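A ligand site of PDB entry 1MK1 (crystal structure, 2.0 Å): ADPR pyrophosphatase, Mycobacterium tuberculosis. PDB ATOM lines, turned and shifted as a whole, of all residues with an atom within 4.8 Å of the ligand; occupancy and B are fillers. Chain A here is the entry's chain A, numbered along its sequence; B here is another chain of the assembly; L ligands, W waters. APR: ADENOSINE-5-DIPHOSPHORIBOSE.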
ATOM      1  N   ALA A  18      28.555  14.769  -4.702  1.00  0.00           N
ATOM      2  CA  ALA A  18      27.226  15.077  -4.202  1.00  0.00           C
ATOM      3  C   ALA A  18      26.644  16.352  -4.810  1.00  0.00           C
ATOM      4  O   ALA A  18      25.542  16.334  -5.379  1.00  0.00           O
ATOM      5  CB  ALA A  18      27.266  15.188  -2.674  1.00  0.00           C
ATOM      6  N   ILE A  19      27.380  17.457  -4.723  1.00  0.00           N
ATOM      7  CA  ILE A  19      26.893  18.731  -5.245  1.00  0.00           C
ATOM      8  C   ILE A  19      27.610  19.274  -6.499  1.00  0.00           C
ATOM      9  O   ILE A  19      27.220  20.324  -7.025  1.00  0.00           O
ATOM     10  CB  ILE A  19      26.923  19.840  -4.150  1.00  0.00           C
ATOM     11  CG1 ILE A  19      28.357  20.211  -3.791  1.00  0.00           C
ATOM     12  CG2 ILE A  19      26.192  19.352  -2.907  1.00  0.00           C
ATOM     13  CD1 ILE A  19      28.450  21.451  -2.934  1.00  0.00           C
ATOM     14  N   PHE A  20      28.646  18.576  -6.965  1.00  0.00           N
ATOM     15  CA  PHE A  20      29.348  19.015  -8.167  1.00  0.00           C
ATOM     16  C   PHE A  20      30.127  17.911  -8.861  1.00  0.00           C
ATOM     17  O   PHE A  20      30.377  16.859  -8.294  1.00  0.00           O
ATOM     18  CB  PHE A  20      30.275  20.208  -7.855  1.00  0.00           C
ATOM     19  CG  PHE A  20      31.384  19.887  -6.890  1.00  0.00           C
ATOM     20  CD1 PHE A  20      32.473  19.109  -7.278  1.00  0.00           C
ATOM     21  CD2 PHE A  20      31.356  20.403  -5.595  1.00  0.00           C
ATOM     22  CE1 PHE A  20      33.522  18.862  -6.395  1.00  0.00           C
ATOM     23  CE2 PHE A  20      32.395  20.161  -4.704  1.00  0.00           C
ATOM     24  CZ  PHE A  20      33.481  19.393  -5.101  1.00  0.00           C
ATOM     25  N   HIS A  42      28.489  22.986 -11.295  1.00  0.00           N
ATOM     26  CA  HIS A  42      27.710  23.239 -10.094  1.00  0.00           C
ATOM     27  C   HIS A  42      26.222  23.434 -10.425  1.00  0.00           C
ATOM     28  O   HIS A  42      25.877  23.705 -11.582  1.00  0.00           O
ATOM     29  CB  HIS A  42      28.296  24.493  -9.425  1.00  0.00           C
ATOM     30  CG  HIS A  42      27.858  24.724  -8.013  1.00  0.00           C
ATOM     31  ND1 HIS A  42      26.688  25.394  -7.693  1.00  0.00           N
ATOM     32  CD2 HIS A  42      28.458  24.432  -6.830  1.00  0.00           C
ATOM     33  CE1 HIS A  42      26.598  25.502  -6.371  1.00  0.00           C
ATOM     34  NE2 HIS A  42      27.651  24.927  -5.827  1.00  0.00           N
ATOM     35  N   ALA A  45      23.059  28.594  -7.383  1.00  0.00           N
ATOM     36  CA  ALA A  45      22.334  28.806  -6.137  1.00  0.00           C
ATOM     37  C   ALA A  45      21.615  30.129  -6.178  1.00  0.00           C
ATOM     38  O   ALA A  45      21.757  30.907  -7.122  1.00  0.00           O
ATOM     39  CB  ALA A  45      23.305  28.758  -4.965  1.00  0.00           C
ATOM     40  N   GLN A  62      26.690  30.728   9.506  1.00  0.00           N
ATOM     41  CA  GLN A  62      26.876  29.317   9.183  1.00  0.00           C
ATOM     42  C   GLN A  62      28.324  28.826   9.064  1.00  0.00           C
ATOM     43  O   GLN A  62      29.184  29.480   8.475  1.00  0.00           O
ATOM     44  CB  GLN A  62      26.125  29.025   7.889  1.00  0.00           C
ATOM     45  CG  GLN A  62      26.278  27.618   7.349  1.00  0.00           C
ATOM     46  CD  GLN A  62      25.133  27.244   6.435  1.00  0.00           C
ATOM     47  OE1 GLN A  62      24.594  28.086   5.722  1.00  0.00           O
ATOM     48  NE2 GLN A  62      24.760  25.964   6.453  1.00  0.00           N
ATOM     49  N   ARG A  64      31.413  26.938   7.699  1.00  0.00           N
ATOM     50  CA  ARG A  64      31.859  26.557   6.368  1.00  0.00           C
ATOM     51  C   ARG A  64      33.119  25.686   6.514  1.00  0.00           C
ATOM     52  O   ARG A  64      34.187  26.170   6.872  1.00  0.00           O
ATOM     53  CB  ARG A  64      32.165  27.807   5.517  1.00  0.00           C
ATOM     54  CG  ARG A  64      30.920  28.572   5.106  1.00  0.00           C
ATOM     55  CD  ARG A  64      29.968  27.680   4.321  1.00  0.00           C
ATOM     56  NE  ARG A  64      28.759  28.368   3.902  1.00  0.00           N
ATOM     57  CZ  ARG A  64      27.758  27.782   3.247  1.00  0.00           C
ATOM     58  NH1 ARG A  64      27.808  26.492   2.925  1.00  0.00           N
ATOM     59  NH2 ARG A  64      26.690  28.498   2.898  1.00  0.00           N
ATOM     60  N   GLU A  73      26.394  35.151   6.412  1.00  0.00           N
ATOM     61  CA  GLU A  73      25.891  35.080   5.046  1.00  0.00           C
ATOM     62  C   GLU A  73      24.413  35.409   4.886  1.00  0.00           C
ATOM     63  O   GLU A  73      23.671  35.525   5.856  1.00  0.00           O
ATOM     64  CB  GLU A  73      26.095  33.678   4.496  1.00  0.00           C
ATOM     65  CG  GLU A  73      27.252  32.921   5.120  1.00  0.00           C
ATOM     66  CD  GLU A  73      27.417  31.535   4.535  1.00  0.00           C
ATOM     67  OE1 GLU A  73      26.431  30.778   4.515  1.00  0.00           O
ATOM     68  OE2 GLU A  73      28.550  31.201   4.100  1.00  0.00           O
ATOM     69  N   ALA A  76      20.663  31.296   1.771  1.00  0.00           N
ATOM     70  CA  ALA A  76      20.881  30.826   0.415  1.00  0.00           C
ATOM     71  C   ALA A  76      20.788  29.301   0.298  1.00  0.00           C
ATOM     72  O   ALA A  76      20.912  28.568   1.294  1.00  0.00           O
ATOM     73  CB  ALA A  76      22.255  31.307  -0.082  1.00  0.00           C
ATOM     74  N   GLY A  77      20.560  28.828  -0.925  1.00  0.00           N
ATOM     75  CA  GLY A  77      20.447  27.409  -1.177  1.00  0.00           C
ATOM     76  C   GLY A  77      20.792  27.035  -2.618  1.00  0.00           C
ATOM     77  O   GLY A  77      20.734  27.877  -3.528  1.00  0.00           O
ATOM     78  N   LEU A  78      21.161  25.777  -2.813  1.00  0.00           N
ATOM     79  CA  LEU A  78      21.517  25.261  -4.122  1.00  0.00           C
ATOM     80  C   LEU A  78      20.280  25.038  -4.984  1.00  0.00           C
ATOM     81  O   LEU A  78      19.187  24.792  -4.450  1.00  0.00           O
ATOM     82  CB  LEU A  78      22.246  23.930  -3.977  1.00  0.00           C
ATOM     83  CG  LEU A  78      23.532  23.910  -3.136  1.00  0.00           C
ATOM     84  CD1 LEU A  78      24.018  22.479  -2.981  1.00  0.00           C
ATOM     85  CD2 LEU A  78      24.592  24.752  -3.817  1.00  0.00           C
ATOM     86  N   ASP A  80      19.162  22.622  -6.474  1.00  0.00           N
ATOM     87  CA  ASP A  80      19.217  21.176  -6.615  1.00  0.00           C
ATOM     88  C   ASP A  80      17.871  20.505  -6.824  1.00  0.00           C
ATOM     89  O   ASP A  80      17.743  19.285  -6.680  1.00  0.00           O
ATOM     90  CB  ASP A  80      19.880  20.550  -5.395  1.00  0.00           C
ATOM     91  CG  ASP A  80      19.190  20.934  -4.103  1.00  0.00           C
ATOM     92  OD1 ASP A  80      17.969  21.184  -4.141  1.00  0.00           O
ATOM     93  OD2 ASP A  80      19.867  20.959  -3.060  1.00  0.00           O
ATOM     94  N   GLU A  93      13.841  28.863   0.702  1.00  0.00           N
ATOM     95  CA  GLU A  93      15.009  29.089   1.546  1.00  0.00           C
ATOM     96  C   GLU A  93      14.777  30.221   2.556  1.00  0.00           C
ATOM     97  O   GLU A  93      15.121  30.101   3.725  1.00  0.00           O
ATOM     98  CB  GLU A  93      16.242  29.393   0.683  1.00  0.00           C
ATOM     99  CG  GLU A  93      17.594  29.300   1.405  1.00  0.00           C
ATOM    100  CD  GLU A  93      17.853  27.920   2.010  1.00  0.00           C
ATOM    101  OE1 GLU A  93      17.609  26.897   1.324  1.00  0.00           O
ATOM    102  OE2 GLU A  93      18.338  27.859   3.169  1.00  0.00           O
ATOM    103  N   GLU A 120      29.605  27.750 -11.484  1.00  0.00           N
ATOM    104  CA  GLU A 120      28.592  28.213 -10.547  1.00  0.00           C
ATOM    105  C   GLU A 120      28.276  29.691 -10.714  1.00  0.00           C
ATOM    106  O   GLU A 120      29.165  30.534 -10.869  1.00  0.00           O
ATOM    107  CB  GLU A 120      29.003  27.990  -9.096  1.00  0.00           C
ATOM    108  CG  GLU A 120      27.963  28.630  -8.184  1.00  0.00           C
ATOM    109  CD  GLU A 120      28.324  28.646  -6.727  1.00  0.00           C
ATOM    110  OE1 GLU A 120      29.433  29.100  -6.360  1.00  0.00           O
ATOM    111  OE2 GLU A 120      27.474  28.225  -5.925  1.00  0.00           O
ATOM    112  N   VAL A 122      25.324  32.615  -9.069  1.00  0.00           N
ATOM    113  CA  VAL A 122      24.332  32.794  -8.018  1.00  0.00           C
ATOM    114  C   VAL A 122      23.470  34.022  -8.254  1.00  0.00           C
ATOM    115  O   VAL A 122      23.989  35.113  -8.539  1.00  0.00           O
ATOM    116  CB  VAL A 122      25.031  32.909  -6.654  1.00  0.00           C
ATOM    117  CG1 VAL A 122      24.010  33.013  -5.549  1.00  0.00           C
ATOM    118  CG2 VAL A 122      25.933  31.717  -6.435  1.00  0.00           C
ATOM    119  N   ASN A 166      31.848  36.219   2.779  1.00  0.00           N
ATOM    120  CA  ASN A 166      31.148  35.364   1.821  1.00  0.00           C
ATOM    121  C   ASN A 166      30.862  36.255   0.598  1.00  0.00           C
ATOM    122  O   ASN A 166      30.233  37.295   0.725  1.00  0.00           O
ATOM    123  CB  ASN A 166      29.841  34.864   2.466  1.00  0.00           C
ATOM    124  CG  ASN A 166      28.969  34.057   1.526  1.00  0.00           C
ATOM    125  OD1 ASN A 166      28.512  34.564   0.507  1.00  0.00           O
ATOM    126  ND2 ASN A 166      28.732  32.796   1.870  1.00  0.00           N
ATOM    127  N   ILE A 168      28.815  36.074  -1.923  1.00  0.00           N
ATOM    128  CA  ILE A 168      27.410  36.277  -2.249  1.00  0.00           C
ATOM    129  C   ILE A 168      26.807  37.346  -1.341  1.00  0.00           C
ATOM    130  O   ILE A 168      26.044  38.210  -1.782  1.00  0.00           O
ATOM    131  CB  ILE A 168      26.630  34.965  -2.068  1.00  0.00           C
ATOM    132  CG1 ILE A 168      27.186  33.916  -3.046  1.00  0.00           C
ATOM    133  CG2 ILE A 168      25.137  35.207  -2.284  1.00  0.00           C
ATOM    134  CD1 ILE A 168      26.806  32.494  -2.723  1.00  0.00           C
ATOM    135  N   THR B  36      29.846  13.851   4.344  1.00  0.00           N
ATOM    136  CA  THR B  36      30.883  13.906   3.328  1.00  0.00           C
ATOM    137  C   THR B  36      30.974  15.381   2.918  1.00  0.00           C
ATOM    138  O   THR B  36      29.950  16.043   2.731  1.00  0.00           O
ATOM    139  CB  THR B  36      30.529  13.057   2.069  1.00  0.00           C
ATOM    140  OG1 THR B  36      30.729  11.674   2.352  1.00  0.00           O
ATOM    141  CG2 THR B  36      31.405  13.464   0.866  1.00  0.00           C
ATOM    142  N   ARG B  37      32.197  15.880   2.792  1.00  0.00           N
ATOM    143  CA  ARG B  37      32.439  17.263   2.385  1.00  0.00           C
ATOM    144  C   ARG B  37      33.581  17.308   1.391  1.00  0.00           C
ATOM    145  O   ARG B  37      34.748  17.163   1.767  1.00  0.00           O
ATOM    146  CB  ARG B  37      32.772  18.117   3.603  1.00  0.00           C
ATOM    147  CG  ARG B  37      31.570  18.492   4.441  1.00  0.00           C
ATOM    148  CD  ARG B  37      30.701  19.534   3.736  1.00  0.00           C
ATOM    149  NE  ARG B  37      29.563  19.953   4.559  1.00  0.00           N
ATOM    150  CZ  ARG B  37      28.435  19.257   4.711  1.00  0.00           C
ATOM    151  NH1 ARG B  37      28.249  18.102   4.078  1.00  0.00           N
ATOM    152  NH2 ARG B  37      27.472  19.724   5.490  1.00  0.00           N
ATOM    153  N   GLU B  38      33.272  17.519   0.117  1.00  0.00           N
ATOM    154  CA  GLU B  38      34.299  17.592  -0.909  1.00  0.00           C
ATOM    155  C   GLU B  38      34.790  19.029  -0.996  1.00  0.00           C
ATOM    156  O   GLU B  38      33.997  19.957  -1.033  1.00  0.00           O
ATOM    157  CB  GLU B  38      33.744  17.121  -2.252  1.00  0.00           C
ATOM    158  CG  GLU B  38      33.449  15.626  -2.244  1.00  0.00           C
ATOM    159  CD  GLU B  38      32.406  15.225  -3.280  1.00  0.00           C
ATOM    160  OE1 GLU B  38      32.671  15.398  -4.484  1.00  0.00           O
ATOM    161  OE2 GLU B  38      31.337  14.732  -2.857  1.00  0.00           O
ATOM    162  N   ALA B 114      33.763  30.869  -3.310  1.00  0.00           N
ATOM    163  CA  ALA B 114      32.814  29.766  -3.308  1.00  0.00           C
ATOM    164  C   ALA B 114      32.891  29.020  -1.973  1.00  0.00           C
ATOM    165  O   ALA B 114      33.384  27.902  -1.900  1.00  0.00           O
ATOM    166  CB  ALA B 114      33.139  28.816  -4.448  1.00  0.00           C
ATOM    167  N   PRO B 115      32.371  29.650  -0.893  1.00  0.00           N
ATOM    168  CA  PRO B 115      32.368  29.107   0.470  1.00  0.00           C
ATOM    169  C   PRO B 115      31.870  27.682   0.615  1.00  0.00           C
ATOM    170  O   PRO B 115      32.298  26.960   1.509  1.00  0.00           O
ATOM    171  CB  PRO B 115      31.502  30.097   1.237  1.00  0.00           C
ATOM    172  CG  PRO B 115      31.756  31.380   0.521  1.00  0.00           C
ATOM    173  CD  PRO B 115      31.675  30.941  -0.923  1.00  0.00           C
ATOM    174  N   GLY B 116      30.967  27.262  -0.264  1.00  0.00           N
ATOM    175  CA  GLY B 116      30.437  25.926  -0.173  1.00  0.00           C
ATOM    176  C   GLY B 116      31.280  24.760  -0.699  1.00  0.00           C
ATOM    177  O   GLY B 116      31.068  23.640  -0.254  1.00  0.00           O
ATOM    178  N   PHE B 117      32.220  24.995  -1.610  1.00  0.00           N
ATOM    179  CA  PHE B 117      33.006  23.885  -2.133  1.00  0.00           C
ATOM    180  C   PHE B 117      34.494  24.101  -2.366  1.00  0.00           C
ATOM    181  O   PHE B 117      35.195  23.183  -2.775  1.00  0.00           O
ATOM    182  CB  PHE B 117      32.388  23.362  -3.429  1.00  0.00           C
ATOM    183  CG  PHE B 117      32.340  24.386  -4.528  1.00  0.00           C
ATOM    184  CD1 PHE B 117      31.298  25.301  -4.599  1.00  0.00           C
ATOM    185  CD2 PHE B 117      33.321  24.407  -5.510  1.00  0.00           C
ATOM    186  CE1 PHE B 117      31.224  26.225  -5.639  1.00  0.00           C
ATOM    187  CE2 PHE B 117      33.264  25.320  -6.557  1.00  0.00           C
ATOM    188  CZ  PHE B 117      32.219  26.232  -6.619  1.00  0.00           C
HETATM  189  N1  APR L   1      30.475  18.281  -0.362  1.00  0.00           N
HETATM  190  C2  APR L   1      29.375  17.475  -0.209  1.00  0.00           C
HETATM  191  N3  APR L   1      28.196  18.060   0.170  1.00  0.00           N
HETATM  192  C4  APR L   1      28.114  19.408   0.394  1.00  0.00           C
HETATM  193  C5  APR L   1      29.242  20.211   0.230  1.00  0.00           C
HETATM  194  C6  APR L   1      30.404  19.637  -0.143  1.00  0.00           C
HETATM  195  N6  APR L   1      31.487  20.428  -0.296  1.00  0.00           N
HETATM  196  N7  APR L   1      28.914  21.513   0.502  1.00  0.00           N
HETATM  197  C8  APR L   1      27.596  21.531   0.837  1.00  0.00           C
HETATM  198  N9  APR L   1      27.102  20.242   0.776  1.00  0.00           N
HETATM  199  C1' APR L   1      25.707  19.915   1.096  1.00  0.00           C
HETATM  200  C2' APR L   1      25.052  19.261   2.286  1.00  0.00           C
HETATM  201  O2' APR L   1      24.399  18.121   1.748  1.00  0.00           O
HETATM  202  C3' APR L   1      24.207  20.427   2.686  1.00  0.00           C
HETATM  203  O3' APR L   1      23.244  19.953   3.604  1.00  0.00           O
HETATM  204  O4' APR L   1      24.586  20.407   0.326  1.00  0.00           O
HETATM  205  C4' APR L   1      23.614  20.831   1.325  1.00  0.00           C
HETATM  206  C5' APR L   1      23.519  22.313   1.665  1.00  0.00           C
HETATM  207  O5' APR L   1      22.547  22.865   0.808  1.00  0.00           O
HETATM  208  PA  APR L   1      22.108  24.361   0.739  1.00  0.00           P
HETATM  209  O1A APR L   1      21.639  24.691   2.191  1.00  0.00           O
HETATM  210  O2A APR L   1      21.009  24.299  -0.352  1.00  0.00           O
HETATM  211  O3A APR L   1      23.233  25.349   0.246  1.00  0.00           O
HETATM  212  PB  APR L   1      24.588  25.955   0.699  1.00  0.00           P
HETATM  213  O1B APR L   1      25.666  24.893   1.023  1.00  0.00           O
HETATM  214  O2B APR L   1      24.413  26.851   1.967  1.00  0.00           O
HETATM  215  O5D APR L   1      25.161  26.885  -0.385  1.00  0.00           O
HETATM  216  C5D APR L   1      24.452  27.992  -0.942  1.00  0.00           C
HETATM  217  O4D APR L   1      26.350  29.355  -0.492  1.00  0.00           O
HETATM  218  O1D APR L   1      28.291  30.248  -0.545  1.00  0.00           O
HETATM  219  C1D APR L   1      27.714  28.959  -0.517  1.00  0.00           C
HETATM  220  O2D APR L   1      29.087  28.368  -2.301  1.00  0.00           O
HETATM  221  C2D APR L   1      27.908  27.972  -1.646  1.00  0.00           C
HETATM  222  O3D APR L   1      26.571  28.907  -3.566  1.00  0.00           O
HETATM  223  C3D APR L   1      26.644  28.085  -2.427  1.00  0.00           C
HETATM  224  C4D APR L   1      25.572  28.827  -1.566  1.00  0.00           C
HETATM  225  O   HOH W   1      27.428  24.195  -0.929  1.00  0.00           O
HETATM  226  O   HOH W   2      27.467  15.172   0.600  1.00  0.00           O
HETATM  227  O   HOH W   3      29.724  23.773   2.910  1.00  0.00           O
HETATM  228  O   HOH W   4      19.363  23.864   3.650  1.00  0.00           O
HETATM  229  O   HOH W   5      29.692  30.147  -3.935  1.00  0.00           O
HETATM  230  O   HOH W   6      20.628  25.720   4.531  1.00  0.00           O
HETATM  231  O   HOH W   7      18.781  24.623   1.291  1.00  0.00           O
HETATM  232  O   HOH W   8      28.233  25.166  -3.125  1.00  0.00           O
HETATM  233  O   HOH W   9      25.956  31.773   1.016  1.00  0.00           O
HETATM  234  O   HOH W  10      19.272  21.958  -0.468  1.00  0.00           O
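ND2 of Asn 166 lies within hydrogen-bond range of OE2 of Glu 73, at 2.7 Å.
N of Ala 18 sits at hydrogen-bond distance from OE2 of Glu 38 of chain B (3.3 Å).
The side-chain carboxylate of Glu 120 sits close to a ring nitrogen (NE2) of His 42 (3.3 Å).
OD1 of Asn 166 is in hydrogen-bond range of N of Ile 168 (2.9 Å).
OE1 of Glu 73 sits close to OE1 of Gln 62 (3.5 Å).
OE1 of Glu 73 lies within salt-bridge range of NH2 of Arg 64 (2.8 Å).
A nitrogen (N6) of the ligand is in hydrogen-bond range of the backbone carbonyl oxygen of Gly 116 of chain B, at 3.2 Å.
The backbone NH of Leu 78 sits at hydrogen-bond distance from an oxygen (O2A) of the ligand, at 2.9 Å.
OE2 of Glu 120 sits at hydrogen-bond distance from O3D of the ligand.
An oxygen (O2B) of the ligand lies within salt-bridge range of the guanidinium group (NH2) of Arg 64 (3.0 Å).
The backbone NH (N) of Gly 116 of chain B is in hydrogen-bond range of an oxygen (O2D) of the ligand (3.0 Å).
The backbone NH of Glu 38 of chain B lies within hydrogen-bond range of a nitrogen (N1) of the ligand (2.9 Å).
O of Glu 38 of chain B sits at hydrogen-bond distance from N6 of the ligand, at 2.7 Å.
Merely in contact with the ligand: Ala 18, Ile 19, Ala 45, Gln 62, Ala 76, Gly 77, Asn 166, Ile 168, Thr 36 of chain B, Arg 37 of chain B, Ala 114 of chain B and Pro 115 of chain B.
Hydrophobic or aromatic side chains within 4 Å of the ligand: Ala 18, Ile 19, Ala 45, Leu 78, Ile 168 and Pro 115 of chain B.
Of the 24 residues printed, 17 come within 4 Å of the ligand.
Along chain A the residues within 4 Å of the ligand span positions 18 to 168.
The nearest printed residue that does not touch the ligand is Val 122 (4.1 Å).
Water W5 lies within hydrogen-bond range of an oxygen (O2D) of the ligand (2.5 Å) and the side-chain carboxylate (OE1) of Glu 120 (2.7 Å).
Water W6 bridges an oxygen (O1A) of the ligand (2.7 Å) and the side-chain carboxylate of Glu 93 (3.4 Å).
Water W7 lies within hydrogen-bond range of the side-chain carboxylate (OE1) of Glu 93 (2.6 Å) and an oxygen (O2A) of the ligand (2.8 Å).
Water W9 bridges O4D of the ligand (2.9 Å) and ND2 of Asn 166 (3.1 Å).
Water W2 lies within hydrogen-bond range of a nitrogen (N3) of the ligand and the backbone carbonyl oxygen (O) of Thr 36 of chain B.
Water W3 lies within hydrogen-bond range of NH1 of Arg 64, N7 of the ligand and O of Gly 116 of chain B.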
